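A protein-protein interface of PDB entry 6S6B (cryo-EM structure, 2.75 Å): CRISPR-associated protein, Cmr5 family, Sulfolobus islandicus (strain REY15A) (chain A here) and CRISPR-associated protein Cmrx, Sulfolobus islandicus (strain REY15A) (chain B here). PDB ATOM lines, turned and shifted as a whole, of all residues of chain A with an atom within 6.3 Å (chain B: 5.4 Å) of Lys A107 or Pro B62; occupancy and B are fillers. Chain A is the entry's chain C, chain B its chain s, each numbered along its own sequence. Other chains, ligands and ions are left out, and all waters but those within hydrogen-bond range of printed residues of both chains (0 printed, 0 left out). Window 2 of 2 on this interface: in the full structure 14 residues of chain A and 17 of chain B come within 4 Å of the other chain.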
ATOM      1  N   ILE A 104      23.673  18.196 -14.739  1.00  0.00           N
ATOM      2  CA  ILE A 104      23.698  19.268 -13.755  1.00  0.00           C
ATOM      3  C   ILE A 104      24.668  18.874 -12.656  1.00  0.00           C
ATOM      4  O   ILE A 104      24.659  17.731 -12.191  1.00  0.00           O
ATOM      5  CB  ILE A 104      22.301  19.542 -13.169  1.00  0.00           C
ATOM      6  CG1 ILE A 104      21.324  19.921 -14.277  1.00  0.00           C
ATOM      7  CG2 ILE A 104      22.372  20.644 -12.135  1.00  0.00           C
ATOM      8  CD1 ILE A 104      20.075  20.594 -13.782  1.00  0.00           C
ATOM      9  N   GLU A 105      25.509  19.818 -12.247  1.00  0.00           N
ATOM     10  CA  GLU A 105      26.481  19.548 -11.200  1.00  0.00           C
ATOM     11  C   GLU A 105      25.776  19.255  -9.884  1.00  0.00           C
ATOM     12  O   GLU A 105      24.731  19.831  -9.581  1.00  0.00           O
ATOM     13  CB  GLU A 105      27.429  20.731 -11.039  1.00  0.00           C
ATOM     14  CG  GLU A 105      28.536  20.746 -12.062  1.00  0.00           C
ATOM     15  CD  GLU A 105      29.274  19.427 -12.123  1.00  0.00           C
ATOM     16  OE1 GLU A 105      29.660  18.915 -11.052  1.00  0.00           O
ATOM     17  OE2 GLU A 105      29.467  18.899 -13.239  1.00  0.00           O
ATOM     18  N   GLN A 106      26.359  18.350  -9.101  1.00  0.00           N
ATOM     19  CA  GLN A 106      25.710  17.929  -7.868  1.00  0.00           C
ATOM     20  C   GLN A 106      25.631  19.069  -6.866  1.00  0.00           C
ATOM     21  O   GLN A 106      24.621  19.218  -6.170  1.00  0.00           O
ATOM     22  CB  GLN A 106      26.446  16.739  -7.264  1.00  0.00           C
ATOM     23  CG  GLN A 106      25.796  16.213  -6.006  1.00  0.00           C
ATOM     24  CD  GLN A 106      26.431  14.940  -5.515  1.00  0.00           C
ATOM     25  OE1 GLN A 106      27.254  14.340  -6.203  1.00  0.00           O
ATOM     26  NE2 GLN A 106      26.055  14.515  -4.317  1.00  0.00           N
ATOM     27  N   LYS A 107      26.691  19.874  -6.766  1.00  0.00           N
ATOM     28  CA  LYS A 107      26.677  21.017  -5.858  1.00  0.00           C
ATOM     29  C   LYS A 107      25.500  21.931  -6.156  1.00  0.00           C
ATOM     30  O   LYS A 107      24.727  22.285  -5.259  1.00  0.00           O
ATOM     31  CB  LYS A 107      27.991  21.790  -5.967  1.00  0.00           C
ATOM     32  CG  LYS A 107      29.231  20.928  -5.868  1.00  0.00           C
ATOM     33  CD  LYS A 107      30.422  21.602  -6.504  1.00  0.00           C
ATOM     34  CE  LYS A 107      30.158  21.900  -7.968  1.00  0.00           C
ATOM     35  NZ  LYS A 107      29.869  20.662  -8.743  1.00  0.00           N
ATOM     36  N   PHE A 108      25.346  22.318  -7.421  1.00  0.00           N
ATOM     37  CA  PHE A 108      24.251  23.198  -7.803  1.00  0.00           C
ATOM     38  C   PHE A 108      22.901  22.576  -7.482  1.00  0.00           C
ATOM     39  O   PHE A 108      21.951  23.285  -7.140  1.00  0.00           O
ATOM     40  CB  PHE A 108      24.345  23.525  -9.289  1.00  0.00           C
ATOM     41  CG  PHE A 108      23.319  24.504  -9.755  1.00  0.00           C
ATOM     42  CD1 PHE A 108      23.477  25.853  -9.517  1.00  0.00           C
ATOM     43  CD2 PHE A 108      22.199  24.079 -10.434  1.00  0.00           C
ATOM     44  CE1 PHE A 108      22.537  26.757  -9.945  1.00  0.00           C
ATOM     45  CE2 PHE A 108      21.256  24.981 -10.863  1.00  0.00           C
ATOM     46  CZ  PHE A 108      21.426  26.322 -10.619  1.00  0.00           C
ATOM     47  N   LEU A 109      22.795  21.251  -7.587  1.00  0.00           N
ATOM     48  CA  LEU A 109      21.515  20.594  -7.354  1.00  0.00           C
ATOM     49  C   LEU A 109      21.150  20.606  -5.879  1.00  0.00           C
ATOM     50  O   LEU A 109      20.025  20.955  -5.511  1.00  0.00           O
ATOM     51  CB  LEU A 109      21.554  19.163  -7.882  1.00  0.00           C
ATOM     52  CG  LEU A 109      20.993  18.970  -9.287  1.00  0.00           C
ATOM     53  CD1 LEU A 109      21.086  17.522  -9.692  1.00  0.00           C
ATOM     54  CD2 LEU A 109      19.564  19.454  -9.362  1.00  0.00           C
ATOM     55  N   ILE A 110      22.087  20.212  -5.017  1.00  0.00           N
ATOM     56  CA  ILE A 110      21.824  20.235  -3.582  1.00  0.00           C
ATOM     57  C   ILE A 110      21.585  21.660  -3.113  1.00  0.00           C
ATOM     58  O   ILE A 110      20.663  21.928  -2.333  1.00  0.00           O
ATOM     59  CB  ILE A 110      22.982  19.581  -2.813  1.00  0.00           C
ATOM     60  CG1 ILE A 110      23.187  18.143  -3.283  1.00  0.00           C
ATOM     61  CG2 ILE A 110      22.722  19.630  -1.324  1.00  0.00           C
ATOM     62  CD1 ILE A 110      24.544  17.593  -2.928  1.00  0.00           C
ATOM     63  N   GLN A 111      22.405  22.598  -3.583  1.00  0.00           N
ATOM     64  CA  GLN A 111      22.212  23.990  -3.214  1.00  0.00           C
ATOM     65  C   GLN A 111      20.882  24.529  -3.713  1.00  0.00           C
ATOM     66  O   GLN A 111      20.377  25.511  -3.162  1.00  0.00           O
ATOM     67  CB  GLN A 111      23.360  24.840  -3.753  1.00  0.00           C
ATOM     68  CG  GLN A 111      23.663  26.046  -2.896  1.00  0.00           C
ATOM     69  CD  GLN A 111      23.849  25.672  -1.442  1.00  0.00           C
ATOM     70  OE1 GLN A 111      22.990  25.942  -0.605  1.00  0.00           O
ATOM     71  NE2 GLN A 111      24.972  25.039  -1.134  1.00  0.00           N
ATOM     72  N   ALA A 112      20.304  23.910  -4.739  1.00  0.00           N
ATOM     73  CA  ALA A 112      18.992  24.330  -5.209  1.00  0.00           C
ATOM     74  C   ALA A 112      17.901  23.851  -4.264  1.00  0.00           C
ATOM     75  O   ALA A 112      17.081  24.644  -3.792  1.00  0.00           O
ATOM     76  CB  ALA A 112      18.751  23.809  -6.623  1.00  0.00           C
ATOM     77  N   ARG A 114      18.189  22.934  -1.251  1.00  0.00           N
ATOM     78  CA  ARG A 114      18.406  23.358   0.130  1.00  0.00           C
ATOM     79  C   ARG A 114      18.007  24.815   0.331  1.00  0.00           C
ATOM     80  O   ARG A 114      17.131  25.127   1.142  1.00  0.00           O
ATOM     81  CB  ARG A 114      19.870  23.130   0.509  1.00  0.00           C
ATOM     82  CG  ARG A 114      20.246  23.623   1.876  1.00  0.00           C
ATOM     83  CD  ARG A 114      21.698  23.318   2.144  1.00  0.00           C
ATOM     84  NE  ARG A 114      21.910  21.930   2.537  1.00  0.00           N
ATOM     85  CZ  ARG A 114      23.077  21.302   2.442  1.00  0.00           C
ATOM     86  NH1 ARG A 114      24.133  21.938   1.961  1.00  0.00           N
ATOM     87  NH2 ARG A 114      23.188  20.040   2.827  1.00  0.00           N
ATOM     88  N   THR B  45      27.936  22.408   7.059  1.00  0.00           N
ATOM     89  CA  THR B  45      28.220  22.170   5.654  1.00  0.00           C
ATOM     90  C   THR B  45      29.446  22.967   5.237  1.00  0.00           C
ATOM     91  O   THR B  45      29.592  24.136   5.602  1.00  0.00           O
ATOM     92  CB  THR B  45      27.023  22.553   4.783  1.00  0.00           C
ATOM     93  OG1 THR B  45      25.817  22.097   5.407  1.00  0.00           O
ATOM     94  CG2 THR B  45      27.145  21.920   3.410  1.00  0.00           C
ATOM     95  N   GLY B  46      30.329  22.325   4.481  1.00  0.00           N
ATOM     96  CA  GLY B  46      31.545  22.957   4.022  1.00  0.00           C
ATOM     97  C   GLY B  46      32.773  22.690   4.859  1.00  0.00           C
ATOM     98  O   GLY B  46      33.791  23.363   4.662  1.00  0.00           O
ATOM     99  N   LEU B  60      35.774  24.085   0.849  1.00  0.00           N
ATOM    100  CA  LEU B  60      34.959  24.920  -0.021  1.00  0.00           C
ATOM    101  C   LEU B  60      33.813  24.181  -0.696  1.00  0.00           C
ATOM    102  O   LEU B  60      32.900  24.836  -1.206  1.00  0.00           O
ATOM    103  CB  LEU B  60      35.826  25.577  -1.107  1.00  0.00           C
ATOM    104  CG  LEU B  60      36.974  26.472  -0.634  1.00  0.00           C
ATOM    105  CD1 LEU B  60      37.521  27.285  -1.794  1.00  0.00           C
ATOM    106  CD2 LEU B  60      36.532  27.384   0.498  1.00  0.00           C
ATOM    107  N   ASP B  61      33.839  22.853  -0.718  1.00  0.00           N
ATOM    108  CA  ASP B  61      32.745  22.091  -1.298  1.00  0.00           C
ATOM    109  C   ASP B  61      31.497  22.224  -0.425  1.00  0.00           C
ATOM    110  O   ASP B  61      31.589  22.177   0.803  1.00  0.00           O
ATOM    111  CB  ASP B  61      33.148  20.616  -1.429  1.00  0.00           C
ATOM    112  CG  ASP B  61      32.289  19.847  -2.422  1.00  0.00           C
ATOM    113  OD1 ASP B  61      31.081  20.129  -2.530  1.00  0.00           O
ATOM    114  OD2 ASP B  61      32.830  18.948  -3.101  1.00  0.00           O
ATOM    115  N   PRO B  62      30.326  22.440  -1.022  1.00  0.00           N
ATOM    116  CA  PRO B  62      29.074  22.337  -0.263  1.00  0.00           C
ATOM    117  C   PRO B  62      28.490  20.933  -0.193  1.00  0.00           C
ATOM    118  O   PRO B  62      27.442  20.755   0.438  1.00  0.00           O
ATOM    119  CB  PRO B  62      28.138  23.275  -1.037  1.00  0.00           C
ATOM    120  CG  PRO B  62      28.644  23.243  -2.426  1.00  0.00           C
ATOM    121  CD  PRO B  62      30.131  23.064  -2.341  1.00  0.00           C
ATOM    122  N   CYS B  63      29.128  19.937  -0.812  1.00  0.00           N
ATOM    123  CA  CYS B  63      28.627  18.569  -0.764  1.00  0.00           C
ATOM    124  C   CYS B  63      29.197  17.756   0.388  1.00  0.00           C
ATOM    125  O   CYS B  63      28.608  16.732   0.750  1.00  0.00           O
ATOM    126  CB  CYS B  63      28.919  17.847  -2.081  1.00  0.00           C
ATOM    127  SG  CYS B  63      28.186  18.638  -3.522  1.00  0.00           S
ATOM    128  N   ASP B  64      30.315  18.174   0.972  1.00  0.00           N
ATOM    129  CA  ASP B  64      30.854  17.512   2.148  1.00  0.00           C
ATOM    130  C   ASP B  64      30.374  18.232   3.401  1.00  0.00           C
ATOM    131  O   ASP B  64      30.181  19.449   3.402  1.00  0.00           O
ATOM    132  CB  ASP B  64      32.384  17.472   2.111  1.00  0.00           C
ATOM    133  CG  ASP B  64      32.989  18.772   1.649  1.00  0.00           C
ATOM    134  OD1 ASP B  64      34.212  18.811   1.402  1.00  0.00           O
ATOM    135  OD2 ASP B  64      32.241  19.759   1.536  1.00  0.00           O
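Of the 10 printed residues of chain A, 4 touch a printed residue of chain B. Hydrophobic or aromatic side chains of chain A that line the printed part of chain B: Ile A110. Along chain A the printed residues that touch a printed residue of chain B span positions 107 to 114. Of the 7 printed residues of chain B, 4 touch a printed residue of chain A. Printed residues of chain B that touch a printed residue of chain A: Thr B45, Asp B61, Pro B62 and Cys B63. Hydrophobic or aromatic side chains of chain B that line the printed part of chain A: Pro B62. Among the printed residues, 7 pairs touch across the chains.
SG of Cys B63 sits close to N of Lys A107 (3.8 Å).
The side-chain carboxylate of Glu A105 is in salt-bridge range of the side-chain amino group of Lys A107, at 2.9 Å. OD1 of Asp B61 sits at hydrogen-bond distance from N of Cys B63 (2.6 Å). O of Asp B61 sits close to OD2 of Asp B64 (2.6 Å).
Printed residues of chain A within 4 Å of Pro B62: Lys A107 (3.9 Å), Gln A111 (3.6 Å) and Arg A114 (3.8 Å). Printed residues of chain B within 4 Å of Ile A110: Cys B63 (3.8 Å). Of the printed residues of chain A, Asp B61 touches Lys A107 (3.9 Å). Of the printed residues of chain A, Cys B63 touches Lys A107 and Ile A110. Ala A112 touches none of the printed residues of chain B. Gly B46 touches none of the printed residues of chain A. The nearest printed residue of chain B that does not touch Lys A107 is Leu B60 (6.7 Å). The nearest residue of chain A that does not touch Pro B62 is Ile A110 (5.2 Å). The nearest printed residue of chain A that does not touch Asp B61 is Ile A110 (7.0 Å).
CG of Lys A107 touches OD1 of Asp B61 (3.9 Å). Lys A107 touches Pro B62. Cys B63 touches Ile A110. Gln A111 touches Pro B62. Arg A114 touches Thr B45. Pro B62 touches Arg A114 (O to NH1, 3.8 Å).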
